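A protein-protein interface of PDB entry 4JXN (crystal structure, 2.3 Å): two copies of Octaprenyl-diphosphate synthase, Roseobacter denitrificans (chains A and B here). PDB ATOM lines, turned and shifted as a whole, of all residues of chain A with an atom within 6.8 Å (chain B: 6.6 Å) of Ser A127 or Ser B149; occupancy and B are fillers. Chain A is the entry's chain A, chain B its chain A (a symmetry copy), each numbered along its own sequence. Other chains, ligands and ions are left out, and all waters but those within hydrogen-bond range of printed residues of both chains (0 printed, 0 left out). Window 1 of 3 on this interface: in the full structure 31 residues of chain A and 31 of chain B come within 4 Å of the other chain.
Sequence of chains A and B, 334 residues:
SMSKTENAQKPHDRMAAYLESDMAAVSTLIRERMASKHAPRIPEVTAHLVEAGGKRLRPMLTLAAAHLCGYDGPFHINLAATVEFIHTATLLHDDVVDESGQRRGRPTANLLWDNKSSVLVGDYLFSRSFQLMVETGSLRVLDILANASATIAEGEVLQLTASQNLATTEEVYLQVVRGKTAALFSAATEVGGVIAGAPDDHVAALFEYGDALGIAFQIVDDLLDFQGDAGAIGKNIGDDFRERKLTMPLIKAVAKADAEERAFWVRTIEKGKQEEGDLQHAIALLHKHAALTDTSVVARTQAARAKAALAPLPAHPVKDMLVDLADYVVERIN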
ATOM      1  N   VAL A 121      11.082 -25.241   9.840  1.00  0.00           N
ATOM      2  CA  VAL A 121      10.592 -26.551   9.412  1.00  0.00           C
ATOM      3  C   VAL A 121       9.841 -27.225  10.564  1.00  0.00           C
ATOM      4  O   VAL A 121       8.770 -27.782  10.358  1.00  0.00           O
ATOM      5  CB  VAL A 121      11.733 -27.448   8.885  1.00  0.00           C
ATOM      6  CG1 VAL A 121      11.260 -28.885   8.707  1.00  0.00           C
ATOM      7  CG2 VAL A 121      12.254 -26.916   7.557  1.00  0.00           C
ATOM      8  N   GLY A 122      10.404 -27.170  11.769  1.00  0.00           N
ATOM      9  CA  GLY A 122       9.720 -27.639  12.981  1.00  0.00           C
ATOM     10  C   GLY A 122       8.385 -26.936  13.175  1.00  0.00           C
ATOM     11  O   GLY A 122       7.348 -27.581  13.366  1.00  0.00           O
ATOM     12  N   ASP A 123       8.406 -25.608  13.101  1.00  0.00           N
ATOM     13  CA  ASP A 123       7.178 -24.813  13.213  1.00  0.00           C
ATOM     14  C   ASP A 123       6.135 -25.284  12.219  1.00  0.00           C
ATOM     15  O   ASP A 123       4.942 -25.345  12.534  1.00  0.00           O
ATOM     16  CB  ASP A 123       7.463 -23.325  12.993  1.00  0.00           C
ATOM     17  CG  ASP A 123       8.225 -22.700  14.139  1.00  0.00           C
ATOM     18  OD1 ASP A 123       8.306 -23.334  15.214  1.00  0.00           O
ATOM     19  OD2 ASP A 123       8.746 -21.575  13.968  1.00  0.00           O
ATOM     20  N   TYR A 124       6.595 -25.636  11.022  1.00  0.00           N
ATOM     21  CA  TYR A 124       5.720 -26.172   9.993  1.00  0.00           C
ATOM     22  C   TYR A 124       5.071 -27.479  10.435  1.00  0.00           C
ATOM     23  O   TYR A 124       3.868 -27.689  10.229  1.00  0.00           O
ATOM     24  CB  TYR A 124       6.470 -26.370   8.658  1.00  0.00           C
ATOM     25  CG  TYR A 124       5.579 -26.932   7.558  1.00  0.00           C
ATOM     26  CD1 TYR A 124       4.344 -26.344   7.270  1.00  0.00           C
ATOM     27  CD2 TYR A 124       5.952 -28.063   6.824  1.00  0.00           C
ATOM     28  CE1 TYR A 124       3.514 -26.853   6.285  1.00  0.00           C
ATOM     29  CE2 TYR A 124       5.125 -28.577   5.832  1.00  0.00           C
ATOM     30  CZ  TYR A 124       3.907 -27.967   5.572  1.00  0.00           C
ATOM     31  OH  TYR A 124       3.071 -28.455   4.603  1.00  0.00           O
ATOM     32  N   LEU A 125       5.858 -28.349  11.055  1.00  0.00           N
ATOM     33  CA  LEU A 125       5.339 -29.652  11.511  1.00  0.00           C
ATOM     34  C   LEU A 125       4.359 -29.484  12.663  1.00  0.00           C
ATOM     35  O   LEU A 125       3.334 -30.176  12.708  1.00  0.00           O
ATOM     36  CB  LEU A 125       6.468 -30.581  11.942  1.00  0.00           C
ATOM     37  CG  LEU A 125       7.579 -30.903  10.938  1.00  0.00           C
ATOM     38  CD1 LEU A 125       8.603 -31.803  11.615  1.00  0.00           C
ATOM     39  CD2 LEU A 125       7.065 -31.541   9.654  1.00  0.00           C
ATOM     40  N   PHE A 126       4.672 -28.560  13.580  1.00  0.00           N
ATOM     41  CA  PHE A 126       3.745 -28.183  14.647  1.00  0.00           C
ATOM     42  C   PHE A 126       2.409 -27.750  14.052  1.00  0.00           C
ATOM     43  O   PHE A 126       1.363 -28.269  14.428  1.00  0.00           O
ATOM     44  CB  PHE A 126       4.271 -27.015  15.495  1.00  0.00           C
ATOM     45  CG  PHE A 126       5.393 -27.361  16.440  1.00  0.00           C
ATOM     46  CD1 PHE A 126       5.474 -28.602  17.071  1.00  0.00           C
ATOM     47  CD2 PHE A 126       6.350 -26.390  16.759  1.00  0.00           C
ATOM     48  CE1 PHE A 126       6.509 -28.878  17.961  1.00  0.00           C
ATOM     49  CE2 PHE A 126       7.382 -26.663  17.647  1.00  0.00           C
ATOM     50  CZ  PHE A 126       7.463 -27.910  18.248  1.00  0.00           C
ATOM     51  N   SER A 127       2.448 -26.799  13.124  1.00  0.00           N
ATOM     52  CA  SER A 127       1.222 -26.330  12.482  1.00  0.00           C
ATOM     53  C   SER A 127       0.469 -27.505  11.864  1.00  0.00           C
ATOM     54  O   SER A 127      -0.745 -27.629  12.028  1.00  0.00           O
ATOM     55  CB  SER A 127       1.524 -25.261  11.422  1.00  0.00           C
ATOM     56  OG  SER A 127       2.310 -25.771  10.363  1.00  0.00           O
ATOM     57  N   ARG A 128       1.192 -28.383  11.174  1.00  0.00           N
ATOM     58  CA  ARG A 128       0.576 -29.566  10.570  1.00  0.00           C
ATOM     59  C   ARG A 128       0.018 -30.534  11.620  1.00  0.00           C
ATOM     60  O   ARG A 128      -1.058 -31.107  11.430  1.00  0.00           O
ATOM     61  CB  ARG A 128       1.572 -30.283   9.665  1.00  0.00           C
ATOM     62  CG  ARG A 128       1.882 -29.523   8.388  1.00  0.00           C
ATOM     63  CD  ARG A 128       0.792 -29.716   7.352  1.00  0.00           C
ATOM     64  NE  ARG A 128       0.783 -28.632   6.374  1.00  0.00           N
ATOM     65  CZ  ARG A 128       0.112 -28.660   5.225  1.00  0.00           C
ATOM     66  NH1 ARG A 128      -0.625 -29.716   4.888  1.00  0.00           N
ATOM     67  NH2 ARG A 128       0.180 -27.617   4.405  1.00  0.00           N
ATOM     68  N   SER A 129       0.732 -30.700  12.733  1.00  0.00           N
ATOM     69  CA  SER A 129       0.245 -31.543  13.828  1.00  0.00           C
ATOM     70  C   SER A 129      -1.103 -31.036  14.369  1.00  0.00           C
ATOM     71  O   SER A 129      -1.974 -31.812  14.732  1.00  0.00           O
ATOM     72  CB  SER A 129       1.292 -31.622  14.946  1.00  0.00           C
ATOM     73  OG  SER A 129       1.365 -30.427  15.704  1.00  0.00           O
ATOM     74  N   PHE A 130      -1.258 -29.718  14.373  1.00  0.00           N
ATOM     75  CA  PHE A 130      -2.404 -29.037  14.959  1.00  0.00           C
ATOM     76  C   PHE A 130      -3.640 -29.208  14.073  1.00  0.00           C
ATOM     77  O   PHE A 130      -4.753 -29.489  14.554  1.00  0.00           O
ATOM     78  CB  PHE A 130      -1.998 -27.562  15.165  1.00  0.00           C
ATOM     79  CG  PHE A 130      -3.069 -26.681  15.732  1.00  0.00           C
ATOM     80  CD1 PHE A 130      -4.064 -27.179  16.561  1.00  0.00           C
ATOM     81  CD2 PHE A 130      -3.047 -25.319  15.457  1.00  0.00           C
ATOM     82  CE1 PHE A 130      -5.034 -26.339  17.077  1.00  0.00           C
ATOM     83  CE2 PHE A 130      -4.009 -24.474  15.978  1.00  0.00           C
ATOM     84  CZ  PHE A 130      -5.005 -24.987  16.787  1.00  0.00           C
ATOM     85  N   GLN A 131      -3.421 -29.057  12.774  1.00  0.00           N
ATOM     86  CA  GLN A 131      -4.422 -29.358  11.756  1.00  0.00           C
ATOM     87  C   GLN A 131      -4.996 -30.763  11.883  1.00  0.00           C
ATOM     88  O   GLN A 131      -6.213 -30.941  11.786  1.00  0.00           O
ATOM     89  CB  GLN A 131      -3.807 -29.209  10.364  1.00  0.00           C
ATOM     90  CG  GLN A 131      -3.585 -27.770   9.939  1.00  0.00           C
ATOM     91  CD  GLN A 131      -3.021 -27.663   8.534  1.00  0.00           C
ATOM     92  OE1 GLN A 131      -1.959 -28.221   8.221  1.00  0.00           O
ATOM     93  NE2 GLN A 131      -3.731 -26.937   7.677  1.00  0.00           N
ATOM     94  N   LEU A 132      -4.114 -31.750  12.067  1.00  0.00           N
ATOM     95  CA  LEU A 132      -4.524 -33.163  12.244  1.00  0.00           C
ATOM     96  C   LEU A 132      -5.406 -33.409  13.479  1.00  0.00           C
ATOM     97  O   LEU A 132      -6.429 -34.093  13.383  1.00  0.00           O
ATOM     98  CB  LEU A 132      -3.296 -34.094  12.287  1.00  0.00           C
ATOM     99  CG  LEU A 132      -2.653 -34.380  10.926  1.00  0.00           C
ATOM    100  CD1 LEU A 132      -1.210 -34.857  11.050  1.00  0.00           C
ATOM    101  CD2 LEU A 132      -3.485 -35.397  10.164  1.00  0.00           C
ATOM    102  N   ILE B  86       0.891 -15.822  19.201  1.00  0.00           N
ATOM    103  CA  ILE B  86       1.358 -16.295  17.900  1.00  0.00           C
ATOM    104  C   ILE B  86       2.249 -15.289  17.160  1.00  0.00           C
ATOM    105  O   ILE B  86       3.226 -15.679  16.499  1.00  0.00           O
ATOM    106  CB  ILE B  86       0.168 -16.689  17.008  1.00  0.00           C
ATOM    107  CG1 ILE B  86      -0.473 -17.969  17.552  1.00  0.00           C
ATOM    108  CG2 ILE B  86       0.614 -16.883  15.564  1.00  0.00           C
ATOM    109  CD1 ILE B  86      -1.805 -18.314  16.929  1.00  0.00           C
ATOM    110  N   ILE B 144      -9.581 -22.482  11.985  1.00  0.00           N
ATOM    111  CA  ILE B 144      -9.170 -21.228  11.360  1.00  0.00           C
ATOM    112  C   ILE B 144      -7.732 -20.888  11.748  1.00  0.00           C
ATOM    113  O   ILE B 144      -6.904 -20.641  10.885  1.00  0.00           O
ATOM    114  CB  ILE B 144     -10.160 -20.098  11.708  1.00  0.00           C
ATOM    115  CG1 ILE B 144     -11.489 -20.353  10.968  1.00  0.00           C
ATOM    116  CG2 ILE B 144      -9.592 -18.734  11.338  1.00  0.00           C
ATOM    117  CD1 ILE B 144     -12.645 -19.503  11.436  1.00  0.00           C
ATOM    118  N   LEU B 145      -7.435 -20.938  13.037  1.00  0.00           N
ATOM    119  CA  LEU B 145      -6.090 -20.646  13.525  1.00  0.00           C
ATOM    120  C   LEU B 145      -5.077 -21.760  13.235  1.00  0.00           C
ATOM    121  O   LEU B 145      -3.867 -21.491  13.163  1.00  0.00           O
ATOM    122  CB  LEU B 145      -6.123 -20.336  15.033  1.00  0.00           C
ATOM    123  CG  LEU B 145      -6.669 -18.937  15.364  1.00  0.00           C
ATOM    124  CD1 LEU B 145      -7.004 -18.839  16.842  1.00  0.00           C
ATOM    125  CD2 LEU B 145      -5.702 -17.827  14.946  1.00  0.00           C
ATOM    126  N   ALA B 146      -5.551 -23.001  13.091  1.00  0.00           N
ATOM    127  CA  ALA B 146      -4.658 -24.109  12.709  1.00  0.00           C
ATOM    128  C   ALA B 146      -4.229 -23.941  11.265  1.00  0.00           C
ATOM    129  O   ALA B 146      -3.050 -24.057  10.955  1.00  0.00           O
ATOM    130  CB  ALA B 146      -5.315 -25.467  12.914  1.00  0.00           C
ATOM    131  N   ASN B 147      -5.180 -23.643  10.388  1.00  0.00           N
ATOM    132  CA  ASN B 147      -4.844 -23.395   8.987  1.00  0.00           C
ATOM    133  C   ASN B 147      -4.009 -22.149   8.780  1.00  0.00           C
ATOM    134  O   ASN B 147      -3.143 -22.118   7.909  1.00  0.00           O
ATOM    135  CB  ASN B 147      -6.102 -23.308   8.151  1.00  0.00           C
ATOM    136  CG  ASN B 147      -6.904 -24.596   8.195  1.00  0.00           C
ATOM    137  OD1 ASN B 147      -6.369 -25.665   8.504  1.00  0.00           O
ATOM    138  ND2 ASN B 147      -8.191 -24.502   7.903  1.00  0.00           N
ATOM    139  N   ALA B 148      -4.266 -21.127   9.585  1.00  0.00           N
ATOM    140  CA  ALA B 148      -3.525 -19.884   9.495  1.00  0.00           C
ATOM    141  C   ALA B 148      -2.058 -20.106   9.870  1.00  0.00           C
ATOM    142  O   ALA B 148      -1.154 -19.637   9.181  1.00  0.00           O
ATOM    143  CB  ALA B 148      -4.151 -18.851  10.412  1.00  0.00           C
ATOM    144  N   SER B 149      -1.847 -20.824  10.971  1.00  0.00           N
ATOM    145  CA  SER B 149      -0.515 -21.181  11.446  1.00  0.00           C
ATOM    146  C   SER B 149       0.222 -21.958  10.377  1.00  0.00           C
ATOM    147  O   SER B 149       1.435 -21.836  10.232  1.00  0.00           O
ATOM    148  CB  SER B 149      -0.619 -22.064  12.683  1.00  0.00           C
ATOM    149  OG  SER B 149      -1.082 -23.358  12.314  1.00  0.00           O
ATOM    150  N   ALA B 150      -0.522 -22.777   9.638  1.00  0.00           N
ATOM    151  CA  ALA B 150       0.053 -23.502   8.511  1.00  0.00           C
ATOM    152  C   ALA B 150       0.526 -22.506   7.459  1.00  0.00           C
ATOM    153  O   ALA B 150       1.685 -22.546   7.056  1.00  0.00           O
ATOM    154  CB  ALA B 150      -0.943 -24.495   7.920  1.00  0.00           C
ATOM    155  N   THR B 151      -0.357 -21.598   7.049  1.00  0.00           N
ATOM    156  CA  THR B 151      -0.005 -20.575   6.062  1.00  0.00           C
ATOM    157  C   THR B 151       1.211 -19.761   6.519  1.00  0.00           C
ATOM    158  O   THR B 151       2.163 -19.558   5.754  1.00  0.00           O
ATOM    159  CB  THR B 151      -1.205 -19.664   5.745  1.00  0.00           C
ATOM    160  OG1 THR B 151      -2.330 -20.477   5.380  1.00  0.00           O
ATOM    161  CG2 THR B 151      -0.890 -18.722   4.582  1.00  0.00           C
ATOM    162  N   ILE B 152       1.207 -19.334   7.774  1.00  0.00           N
ATOM    163  CA  ILE B 152       2.292 -18.492   8.273  1.00  0.00           C
ATOM    164  C   ILE B 152       3.630 -19.203   8.135  1.00  0.00           C
ATOM    165  O   ILE B 152       4.563 -18.687   7.498  1.00  0.00           O
ATOM    166  CB  ILE B 152       2.069 -18.079   9.738  1.00  0.00           C
ATOM    167  CG1 ILE B 152       0.865 -17.137   9.835  1.00  0.00           C
ATOM    168  CG2 ILE B 152       3.313 -17.401  10.312  1.00  0.00           C
ATOM    169  CD1 ILE B 152       0.159 -17.194  11.169  1.00  0.00           C
ATOM    170  N   ALA B 153       3.711 -20.393   8.724  1.00  0.00           N
ATOM    171  CA  ALA B 153       4.943 -21.186   8.697  1.00  0.00           C
ATOM    172  C   ALA B 153       5.369 -21.529   7.262  1.00  0.00           C
ATOM    173  O   ALA B 153       6.556 -21.583   6.960  1.00  0.00           O
ATOM    174  CB  ALA B 153       4.772 -22.449   9.523  1.00  0.00           C
ATOM    175  N   GLU B 154       4.385 -21.738   6.390  1.00  0.00           N
ATOM    176  CA  GLU B 154       4.605 -22.045   4.975  1.00  0.00           C
ATOM    177  C   GLU B 154       5.172 -20.860   4.204  1.00  0.00           C
ATOM    178  O   GLU B 154       5.967 -21.043   3.287  1.00  0.00           O
ATOM    179  CB  GLU B 154       3.280 -22.477   4.342  1.00  0.00           C
ATOM    180  CG  GLU B 154       3.388 -23.004   2.925  1.00  0.00           C
ATOM    181  CD  GLU B 154       2.106 -23.672   2.432  1.00  0.00           C
ATOM    182  OE1 GLU B 154       1.276 -24.117   3.258  1.00  0.00           O
ATOM    183  OE2 GLU B 154       1.930 -23.768   1.201  1.00  0.00           O
ATOM    184  N   GLU B 156       7.005 -18.369   5.731  1.00  0.00           N
ATOM    185  CA  GLU B 156       8.356 -18.236   6.301  1.00  0.00           C
ATOM    186  C   GLU B 156       9.402 -19.045   5.516  1.00  0.00           C
ATOM    187  O   GLU B 156      10.512 -18.571   5.271  1.00  0.00           O
ATOM    188  CB  GLU B 156       8.373 -18.650   7.788  1.00  0.00           C
ATOM    189  CG  GLU B 156       7.707 -17.672   8.761  1.00  0.00           C
ATOM    190  CD  GLU B 156       7.750 -18.141  10.222  1.00  0.00           C
ATOM    191  OE1 GLU B 156       7.415 -19.311  10.511  1.00  0.00           O
ATOM    192  OE2 GLU B 156       8.109 -17.333  11.104  1.00  0.00           O
ATOM    193  N   ALA B 183      -2.254 -13.486   6.765  1.00  0.00           N
ATOM    194  CA  ALA B 183      -2.969 -14.649   7.287  1.00  0.00           C
ATOM    195  C   ALA B 183      -3.413 -14.454   8.729  1.00  0.00           C
ATOM    196  O   ALA B 183      -4.558 -14.800   9.078  1.00  0.00           O
ATOM    197  CB  ALA B 183      -2.125 -15.908   7.158  1.00  0.00           C
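NE2 of Gln A131 is in hydrogen-bond range of OD1 of Asn B147 (3.0 Å).
The side-chain carboxylate of Glu B154 lies within salt-bridge range of the guanidinium group of Arg A128, 3.8 Å away.
OG of Ser A127 is in hydrogen-bond range of O of Asp A123 (3.4 Å).
O of Asn B147 sits at hydrogen-bond distance from OG1 of Thr B151, at 3.1 Å.
OG of Ser B149 lies close to O of Leu B145 (3.5 Å).
The guanidinium group (NE) of Arg A128 sits close to the side-chain amide oxygen (OE1) of Gln A131 (3.3 Å).
O of Tyr A124 is in hydrogen-bond range of OG of Ser A127 (2.5 Å).
The side-chain hydroxyl of Tyr A124 sits at hydrogen-bond distance from the guanidinium group of Arg A128, 2.9 Å away.
CA of Tyr A124 touches CB of Ala B153, at 3.9 Å.
Ser B149 touches Ser A127.
Ala B150 touches Ser A127.
Ala B146 touches Phe A130 (CA to CE2, 3.4 Å).
Ala B146 touches Gln A131.
Ala B150 touches Gln A131.
Ser A127 touches just these residues of chain B: Ser B149 (3.3 Å) and Ala B150 (3.7 Å).
Ser B149 touches just one residue of chain A: Ser A127.
Printed residues of chain A within 4 Å of Ala B153: Tyr A124.
Of the printed residues of chain A, Glu B154 touches Arg A128 (3.8 Å).
Of the printed residues of chain B, Arg A128 touches Glu B154.
Thr B151 touches none of the printed residues of chain A.
Val A121 touches none of the printed residues of chain B.
The nearest residue of chain B that does not touch Ser A127 is Ala B153 (4.2 Å).
The nearest printed residue of chain A that does not touch Glu B154 is Tyr A124 (4.7 Å).
Of the 12 printed residues of chain A, 5 touch a printed residue of chain B.
Printed residues of chain A that touch a printed residue of chain B: Tyr A124, Ser A127, Arg A128, Phe A130 and Gln A131.
Hydrophobic or aromatic side chains of chain A that line the printed part of chain B: Phe A130.
Printed residues of chain B that touch a printed residue of chain A: Ala B146, Asn B147, Ser B149, Ala B150, Ala B153 and Glu B154.
No position is printed for both chains.
Of the 8 pairs that touch across the chains among the printed residues, none has its exchanged pair printed and touching as well.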
